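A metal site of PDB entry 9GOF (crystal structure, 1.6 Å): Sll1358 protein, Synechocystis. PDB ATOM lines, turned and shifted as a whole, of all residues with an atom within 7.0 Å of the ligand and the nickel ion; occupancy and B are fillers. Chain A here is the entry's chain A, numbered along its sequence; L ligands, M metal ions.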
ATOM      1  N   LEU A 220      30.440  16.678 -15.689  1.00  0.00           N
ATOM      2  CA  LEU A 220      30.492  16.929 -17.124  1.00  0.00           C
ATOM      3  C   LEU A 220      31.950  17.073 -17.519  1.00  0.00           C
ATOM      4  O   LEU A 220      32.667  17.910 -16.960  1.00  0.00           O
ATOM      5  CB  LEU A 220      29.698  18.188 -17.505  1.00  0.00           C
ATOM      6  CG  LEU A 220      29.996  18.668 -18.923  1.00  0.00           C
ATOM      7  CD1 LEU A 220      29.016  18.021 -19.850  1.00  0.00           C
ATOM      8  CD2 LEU A 220      29.862  20.186 -19.000  1.00  0.00           C
ATOM      9  N   ALA A 237      31.186  15.342 -25.186  1.00  0.00           N
ATOM     10  CA  ALA A 237      31.179  15.457 -23.731  1.00  0.00           C
ATOM     11  C   ALA A 237      30.712  14.160 -23.104  1.00  0.00           C
ATOM     12  O   ALA A 237      29.898  13.434 -23.694  1.00  0.00           O
ATOM     13  CB  ALA A 237      30.282  16.604 -23.258  1.00  0.00           C
ATOM     14  N   ILE A 239      28.701  12.887 -19.706  1.00  0.00           N
ATOM     15  CA  ILE A 239      27.856  13.331 -18.608  1.00  0.00           C
ATOM     16  C   ILE A 239      27.602  12.136 -17.699  1.00  0.00           C
ATOM     17  O   ILE A 239      27.223  11.062 -18.179  1.00  0.00           O
ATOM     18  CB  ILE A 239      26.532  13.950 -19.086  1.00  0.00           C
ATOM     19  CG1 ILE A 239      26.815  15.217 -19.903  1.00  0.00           C
ATOM     20  CG2 ILE A 239      25.619  14.265 -17.896  1.00  0.00           C
ATOM     21  CD1 ILE A 239      25.592  15.777 -20.595  1.00  0.00           C
ATOM     22  N   ARG A 247      20.484  17.104 -15.559  1.00  0.00           N
ATOM     23  CA  ARG A 247      21.145  18.186 -16.280  1.00  0.00           C
ATOM     24  C   ARG A 247      20.080  19.235 -16.539  1.00  0.00           C
ATOM     25  O   ARG A 247      19.025  18.923 -17.096  1.00  0.00           O
ATOM     26  CB  ARG A 247      21.777  17.698 -17.589  1.00  0.00           C
ATOM     27  CG  ARG A 247      22.253  18.821 -18.527  1.00  0.00           C
ATOM     28  CD  ARG A 247      23.577  19.430 -18.061  1.00  0.00           C
ATOM     29  NE  ARG A 247      24.085  20.359 -19.076  1.00  0.00           N
ATOM     30  CZ  ARG A 247      23.789  21.644 -19.146  1.00  0.00           C
ATOM     31  NH1 ARG A 247      23.145  22.268 -18.169  1.00  0.00           N
ATOM     32  NH2 ARG A 247      24.157  22.339 -20.222  1.00  0.00           N
ATOM     33  N   GLN A 248      20.313  20.459 -16.073  1.00  0.00           N
ATOM     34  CA  GLN A 248      19.288  21.511 -16.128  1.00  0.00           C
ATOM     35  C   GLN A 248      18.821  21.810 -17.542  1.00  0.00           C
ATOM     36  O   GLN A 248      19.508  21.561 -18.532  1.00  0.00           O
ATOM     37  CB  GLN A 248      19.803  22.807 -15.496  1.00  0.00           C
ATOM     38  CG  GLN A 248      20.186  22.705 -14.034  1.00  0.00           C
ATOM     39  CD  GLN A 248      20.353  24.087 -13.420  1.00  0.00           C
ATOM     40  OE1 GLN A 248      20.075  25.101 -14.072  1.00  0.00           O
ATOM     41  NE2 GLN A 248      20.745  24.136 -12.152  1.00  0.00           N
ATOM     42  N   HIS A 250      18.168  23.749 -20.798  1.00  0.00           N
ATOM     43  CA  HIS A 250      19.063  24.619 -21.543  1.00  0.00           C
ATOM     44  C   HIS A 250      18.775  24.458 -23.030  1.00  0.00           C
ATOM     45  O   HIS A 250      17.995  23.598 -23.446  1.00  0.00           O
ATOM     46  CB  HIS A 250      20.535  24.297 -21.251  1.00  0.00           C
ATOM     47  CG  HIS A 250      20.978  22.943 -21.746  1.00  0.00           C
ATOM     48  ND1 HIS A 250      20.682  21.773 -21.084  1.00  0.00           N
ATOM     49  CD2 HIS A 250      21.713  22.598 -22.826  1.00  0.00           C
ATOM     50  CE1 HIS A 250      21.204  20.750 -21.739  1.00  0.00           C
ATOM     51  NE2 HIS A 250      21.836  21.227 -22.799  1.00  0.00           N
ATOM     52  N   TRP A 251      19.423  25.306 -23.843  1.00  0.00           N
ATOM     53  CA  TRP A 251      19.477  25.084 -25.273  1.00  0.00           C
ATOM     54  C   TRP A 251      20.859  25.441 -25.792  1.00  0.00           C
ATOM     55  O   TRP A 251      21.650  26.107 -25.116  1.00  0.00           O
ATOM     56  CB  TRP A 251      18.398  25.866 -26.043  1.00  0.00           C
ATOM     57  CG  TRP A 251      18.646  27.363 -26.193  1.00  0.00           C
ATOM     58  CD1 TRP A 251      19.262  27.994 -27.231  1.00  0.00           C
ATOM     59  CD2 TRP A 251      18.232  28.394 -25.277  1.00  0.00           C
ATOM     60  NE1 TRP A 251      19.280  29.360 -27.015  1.00  0.00           N
ATOM     61  CE2 TRP A 251      18.648  29.629 -25.826  1.00  0.00           C
ATOM     62  CE3 TRP A 251      17.543  28.389 -24.059  1.00  0.00           C
ATOM     63  CZ2 TRP A 251      18.403  30.848 -25.184  1.00  0.00           C
ATOM     64  CZ3 TRP A 251      17.311  29.604 -23.412  1.00  0.00           C
ATOM     65  CH2 TRP A 251      17.728  30.816 -23.987  1.00  0.00           C
ATOM     66  N   HIS A 252      21.143  24.974 -27.011  1.00  0.00           N
ATOM     67  CA  HIS A 252      22.376  25.310 -27.725  1.00  0.00           C
ATOM     68  C   HIS A 252      22.057  26.223 -28.894  1.00  0.00           C
ATOM     69  O   HIS A 252      21.325  25.825 -29.814  1.00  0.00           O
ATOM     70  CB  HIS A 252      23.074  24.036 -28.198  1.00  0.00           C
ATOM     71  CG  HIS A 252      23.274  23.072 -27.084  1.00  0.00           C
ATOM     72  ND1 HIS A 252      24.213  23.275 -26.095  1.00  0.00           N
ATOM     73  CD2 HIS A 252      22.603  21.942 -26.745  1.00  0.00           C
ATOM     74  CE1 HIS A 252      24.113  22.304 -25.201  1.00  0.00           C
ATOM     75  NE2 HIS A 252      23.145  21.485 -25.573  1.00  0.00           N
ATOM     76  N   GLU A 257      22.657  18.258 -31.106  1.00  0.00           N
ATOM     77  CA  GLU A 257      23.234  17.411 -30.075  1.00  0.00           C
ATOM     78  C   GLU A 257      22.830  15.964 -30.314  1.00  0.00           C
ATOM     79  O   GLU A 257      21.637  15.643 -30.329  1.00  0.00           O
ATOM     80  CB  GLU A 257      22.778  17.861 -28.679  1.00  0.00           C
ATOM     81  CG  GLU A 257      23.321  17.003 -27.530  1.00  0.00           C
ATOM     82  CD  GLU A 257      22.942  17.552 -26.165  1.00  0.00           C
ATOM     83  OE1 GLU A 257      22.835  18.792 -26.054  1.00  0.00           O
ATOM     84  OE2 GLU A 257      22.724  16.758 -25.230  1.00  0.00           O
ATOM     85  N   GLN A 259      23.243  11.968 -28.952  1.00  0.00           N
ATOM     86  CA  GLN A 259      23.432  11.382 -27.622  1.00  0.00           C
ATOM     87  C   GLN A 259      23.450   9.858 -27.689  1.00  0.00           C
ATOM     88  O   GLN A 259      22.684   9.261 -28.451  1.00  0.00           O
ATOM     89  CB  GLN A 259      22.296  11.800 -26.670  1.00  0.00           C
ATOM     90  CG  GLN A 259      21.968  13.295 -26.739  1.00  0.00           C
ATOM     91  CD  GLN A 259      20.679  13.607 -26.022  1.00  0.00           C
ATOM     92  OE1 GLN A 259      19.733  12.817 -26.066  1.00  0.00           O
ATOM     93  NE2 GLN A 259      20.626  14.747 -25.349  1.00  0.00           N
ATOM     94  N   LEU A 268      14.798  11.940 -21.244  1.00  0.00           N
ATOM     95  CA  LEU A 268      15.100  13.117 -22.055  1.00  0.00           C
ATOM     96  C   LEU A 268      13.802  13.860 -22.322  1.00  0.00           C
ATOM     97  O   LEU A 268      12.795  13.244 -22.681  1.00  0.00           O
ATOM     98  CB  LEU A 268      15.750  12.716 -23.388  1.00  0.00           C
ATOM     99  CG  LEU A 268      15.909  13.836 -24.424  1.00  0.00           C
ATOM    100  CD1 LEU A 268      16.991  14.793 -23.975  1.00  0.00           C
ATOM    101  CD2 LEU A 268      16.264  13.272 -25.800  1.00  0.00           C
ATOM    102  N   VAL A 290      18.872  16.152 -30.316  1.00  0.00           N
ATOM    103  CA  VAL A 290      18.196  17.408 -29.991  1.00  0.00           C
ATOM    104  C   VAL A 290      18.560  18.419 -31.062  1.00  0.00           C
ATOM    105  O   VAL A 290      19.717  18.851 -31.121  1.00  0.00           O
ATOM    106  CB  VAL A 290      18.584  17.920 -28.594  1.00  0.00           C
ATOM    107  CG1 VAL A 290      17.832  19.219 -28.283  1.00  0.00           C
ATOM    108  CG2 VAL A 290      18.287  16.854 -27.539  1.00  0.00           C
ATOM    109  N   TYR A 294      16.524  23.697 -29.745  1.00  0.00           N
ATOM    110  CA  TYR A 294      15.412  23.137 -28.988  1.00  0.00           C
ATOM    111  C   TYR A 294      15.769  23.098 -27.507  1.00  0.00           C
ATOM    112  O   TYR A 294      16.908  22.759 -27.137  1.00  0.00           O
ATOM    113  CB  TYR A 294      15.067  21.736 -29.479  1.00  0.00           C
ATOM    114  CG  TYR A 294      14.311  21.662 -30.788  1.00  0.00           C
ATOM    115  CD1 TYR A 294      14.408  22.670 -31.756  1.00  0.00           C
ATOM    116  CD2 TYR A 294      13.514  20.564 -31.079  1.00  0.00           C
ATOM    117  CE1 TYR A 294      13.727  22.580 -32.958  1.00  0.00           C
ATOM    118  CE2 TYR A 294      12.827  20.467 -32.267  1.00  0.00           C
ATOM    119  CZ  TYR A 294      12.934  21.464 -33.208  1.00  0.00           C
ATOM    120  OH  TYR A 294      12.249  21.344 -34.399  1.00  0.00           O
ATOM    121  N   HIS A 296      15.960  21.558 -23.825  1.00  0.00           N
ATOM    122  CA  HIS A 296      16.027  20.162 -23.400  1.00  0.00           C
ATOM    123  C   HIS A 296      16.610  20.067 -21.994  1.00  0.00           C
ATOM    124  O   HIS A 296      17.219  21.009 -21.485  1.00  0.00           O
ATOM    125  CB  HIS A 296      16.828  19.288 -24.387  1.00  0.00           C
ATOM    126  CG  HIS A 296      18.219  19.787 -24.674  1.00  0.00           C
ATOM    127  ND1 HIS A 296      18.467  20.984 -25.310  1.00  0.00           N
ATOM    128  CD2 HIS A 296      19.432  19.226 -24.439  1.00  0.00           C
ATOM    129  CE1 HIS A 296      19.780  21.140 -25.449  1.00  0.00           C
ATOM    130  NE2 HIS A 296      20.387  20.086 -24.934  1.00  0.00           N
ATOM    131  N   ALA A 297      16.342  18.928 -21.366  1.00  0.00           N
ATOM    132  CA  ALA A 297      16.905  18.579 -20.072  1.00  0.00           C
ATOM    133  C   ALA A 297      17.025  17.064 -20.022  1.00  0.00           C
ATOM    134  O   ALA A 297      16.327  16.353 -20.760  1.00  0.00           O
ATOM    135  CB  ALA A 297      16.067  19.090 -18.894  1.00  0.00           C
ATOM    136  N   ILE A 298      17.899  16.585 -19.146  1.00  0.00           N
ATOM    137  CA  ILE A 298      18.162  15.147 -19.016  1.00  0.00           C
ATOM    138  C   ILE A 298      18.045  14.793 -17.544  1.00  0.00           C
ATOM    139  O   ILE A 298      18.619  15.478 -16.688  1.00  0.00           O
ATOM    140  CB  ILE A 298      19.552  14.765 -19.542  1.00  0.00           C
ATOM    141  CG1 ILE A 298      19.731  15.228 -20.992  1.00  0.00           C
ATOM    142  CG2 ILE A 298      19.737  13.246 -19.413  1.00  0.00           C
ATOM    143  CD1 ILE A 298      21.190  15.153 -21.483  1.00  0.00           C
ATOM    144  N   ILE A 308      26.402   9.082 -20.209  1.00  0.00           N
ATOM    145  CA  ILE A 308      26.088   9.314 -21.605  1.00  0.00           C
ATOM    146  C   ILE A 308      27.238  10.057 -22.278  1.00  0.00           C
ATOM    147  O   ILE A 308      28.007  10.770 -21.632  1.00  0.00           O
ATOM    148  CB  ILE A 308      24.765  10.080 -21.802  1.00  0.00           C
ATOM    149  CG1 ILE A 308      24.932  11.558 -21.450  1.00  0.00           C
ATOM    150  CG2 ILE A 308      23.636   9.459 -20.950  1.00  0.00           C
ATOM    151  CD1 ILE A 308      23.633  12.350 -21.487  1.00  0.00           C
ATOM    152  N   VAL A 310      27.682  12.771 -25.467  1.00  0.00           N
ATOM    153  CA  VAL A 310      26.928  13.664 -26.348  1.00  0.00           C
ATOM    154  C   VAL A 310      27.907  14.359 -27.263  1.00  0.00           C
ATOM    155  O   VAL A 310      29.046  14.663 -26.874  1.00  0.00           O
ATOM    156  CB  VAL A 310      26.062  14.690 -25.562  1.00  0.00           C
ATOM    157  CG1 VAL A 310      25.058  13.961 -24.648  1.00  0.00           C
ATOM    158  CG2 VAL A 310      26.945  15.632 -24.742  1.00  0.00           C
ATOM    159  N   PHE A 312      28.378  17.340 -30.556  1.00  0.00           N
ATOM    160  CA  PHE A 312      27.856  18.548 -31.170  1.00  0.00           C
ATOM    161  C   PHE A 312      28.556  18.783 -32.498  1.00  0.00           C
ATOM    162  O   PHE A 312      29.763  18.555 -32.604  1.00  0.00           O
ATOM    163  CB  PHE A 312      28.061  19.772 -30.272  1.00  0.00           C
ATOM    164  CG  PHE A 312      27.482  19.608 -28.898  1.00  0.00           C
ATOM    165  CD1 PHE A 312      28.234  19.020 -27.890  1.00  0.00           C
ATOM    166  CD2 PHE A 312      26.191  20.012 -28.623  1.00  0.00           C
ATOM    167  CE1 PHE A 312      27.695  18.835 -26.628  1.00  0.00           C
ATOM    168  CE2 PHE A 312      25.650  19.837 -27.370  1.00  0.00           C
ATOM    169  CZ  PHE A 312      26.405  19.259 -26.363  1.00  0.00           C
ATOM    170  N   TYR A 317      31.485  24.913 -27.791  1.00  0.00           N
ATOM    171  CA  TYR A 317      30.333  24.506 -26.989  1.00  0.00           C
ATOM    172  C   TYR A 317      29.624  25.745 -26.469  1.00  0.00           C
ATOM    173  O   TYR A 317      30.221  26.568 -25.772  1.00  0.00           O
ATOM    174  CB  TYR A 317      30.756  23.611 -25.838  1.00  0.00           C
ATOM    175  CG  TYR A 317      29.631  23.228 -24.890  1.00  0.00           C
ATOM    176  CD1 TYR A 317      28.718  22.237 -25.226  1.00  0.00           C
ATOM    177  CD2 TYR A 317      29.499  23.848 -23.646  1.00  0.00           C
ATOM    178  CE1 TYR A 317      27.700  21.867 -24.354  1.00  0.00           C
ATOM    179  CE2 TYR A 317      28.484  23.487 -22.775  1.00  0.00           C
ATOM    180  CZ  TYR A 317      27.578  22.504 -23.125  1.00  0.00           C
ATOM    181  OH  TYR A 317      26.571  22.140 -22.258  1.00  0.00           O
ATOM    182  N   GLN A 318      28.351  25.895 -26.832  1.00  0.00           N
ATOM    183  CA  GLN A 318      27.543  27.041 -26.414  1.00  0.00           C
ATOM    184  C   GLN A 318      26.262  26.513 -25.793  1.00  0.00           C
ATOM    185  O   GLN A 318      25.508  25.785 -26.448  1.00  0.00           O
ATOM    186  CB  GLN A 318      27.212  27.946 -27.601  1.00  0.00           C
ATOM    187  CG  GLN A 318      28.400  28.730 -28.142  1.00  0.00           C
ATOM    188  CD  GLN A 318      28.030  29.585 -29.324  1.00  0.00           C
ATOM    189  OE1 GLN A 318      26.847  29.887 -29.529  1.00  0.00           O
ATOM    190  NE2 GLN A 318      29.024  30.012 -30.100  1.00  0.00           N
ATOM    191  N   SER A 319      26.012  26.908 -24.552  1.00  0.00           N
ATOM    192  CA  SER A 319      24.794  26.503 -23.852  1.00  0.00           C
ATOM    193  C   SER A 319      24.261  27.695 -23.087  1.00  0.00           C
ATOM    194  O   SER A 319      25.032  28.418 -22.442  1.00  0.00           O
ATOM    195  CB  SER A 319      25.082  25.331 -22.902  1.00  0.00           C
ATOM    196  OG  SER A 319      24.013  25.095 -21.993  1.00  0.00           O
ATOM    197  N   ASP A 321      21.709  28.009 -20.126  1.00  0.00           N
ATOM    198  CA  ASP A 321      20.833  27.371 -19.146  1.00  0.00           C
ATOM    199  C   ASP A 321      19.698  28.302 -18.772  1.00  0.00           C
ATOM    200  O   ASP A 321      19.894  29.520 -18.659  1.00  0.00           O
ATOM    201  CB  ASP A 321      21.604  26.986 -17.883  1.00  0.00           C
ATOM    202  CG  ASP A 321      22.572  25.835 -18.112  1.00  0.00           C
ATOM    203  OD1 ASP A 321      22.197  24.852 -18.756  1.00  0.00           O
ATOM    204  OD2 ASP A 321      23.725  25.910 -17.636  1.00  0.00           O
ATOM    205  N   ILE A 354      24.351  24.111 -13.240  1.00  0.00           N
ATOM    206  CA  ILE A 354      24.500  23.197 -14.394  1.00  0.00           C
ATOM    207  C   ILE A 354      23.675  21.936 -14.211  1.00  0.00           C
ATOM    208  O   ILE A 354      22.936  21.520 -15.107  1.00  0.00           O
ATOM    209  CB  ILE A 354      25.964  22.822 -14.676  1.00  0.00           C
ATOM    210  CG1 ILE A 354      26.803  24.098 -14.887  1.00  0.00           C
ATOM    211  CG2 ILE A 354      26.043  21.865 -15.865  1.00  0.00           C
ATOM    212  CD1 ILE A 354      26.356  24.903 -16.067  1.00  0.00           C
HETATM  213  N1  LIG L   1      22.230  18.160 -23.230  1.00  0.00           N
HETATM  214  C1  LIG L   1      23.369  18.062 -22.334  1.00  0.00           C
HETATM  215  C2  LIG L   1      24.399  19.153 -22.533  1.00  0.00           C
HETATM  216  O1  LIG L   1      25.209  19.410 -21.642  1.00  0.00           O
HETATM  217  O2  LIG L   1      24.463  19.819 -23.580  1.00  0.00           O
HETATM  218 NI    NI M   1      22.459  19.952 -24.404  1.00  0.00          NI
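The side-chain carboxylate of Glu 257 sits at hydrogen-bond distance from the side-chain amide nitrogen of Gln 259 (2.9 Å). ND1 of His 296 lies within hydrogen-bond range of O of Tyr 294, 3.0 Å away. The guanidinium group of Arg 247 sits at hydrogen-bond distance from the side-chain hydroxyl of Ser 319. The backbone carbonyl oxygen of Gln 248 is in hydrogen-bond range of a ring nitrogen (ND1) of His 250 (2.8 Å). NH1 of Arg 247 sits at hydrogen-bond distance from O of Ile 354. O of Ile 298 lies within hydrogen-bond range of N of Arg 247, 2.7 Å away. A ring nitrogen (ND1) of His 252 sits at hydrogen-bond distance from the backbone carbonyl oxygen of Gln 318. The backbone carbonyl oxygen (O) of Glu 257 lies within hydrogen-bond range of the backbone NH (N) of Val 290 (2.8 Å).
The side-chain hydroxyl (OH) of Tyr 317 is in hydrogen-bond range of an oxygen (O1) of the ligand (3.1 Å). An oxygen (O1) of the ligand is in salt-bridge range of the guanidinium group of Arg 247, 3.0 Å away.
Of the 24 residues printed, 4 come within 4 Å of the nickel ion. The nearest printed residue that does not touch the nickel ion is Phe 312 (4.4 Å).
The nickel ion is bound by NE2 of His 252 (2.0 Å), OE1 of Glu 257 (2.1 Å), NE2 of His 250 (2.1 Å), NE2 of His 296 (2.1 Å), N1 of the ligand (2.2 Å) and O2 of the ligand (2.2 Å).
Ile 239 touches the ligand (CD1 to C1, 3.6 Å). Ile 298 touches the ligand. CZ of Phe 312 touches O2 of the ligand (3.4 Å). Hydrophobic or aromatic side chains within 4 Å of the ligand: Ile 239, His 250, His 252, His 296, Ile 298, Phe 312 and Tyr 317. Nine residues have an atom within 4 Å of the ligand: Ile 239, Arg 247, His 250, His 252, Glu 257, His 296, Ile 298, Phe 312 and Tyr 317.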
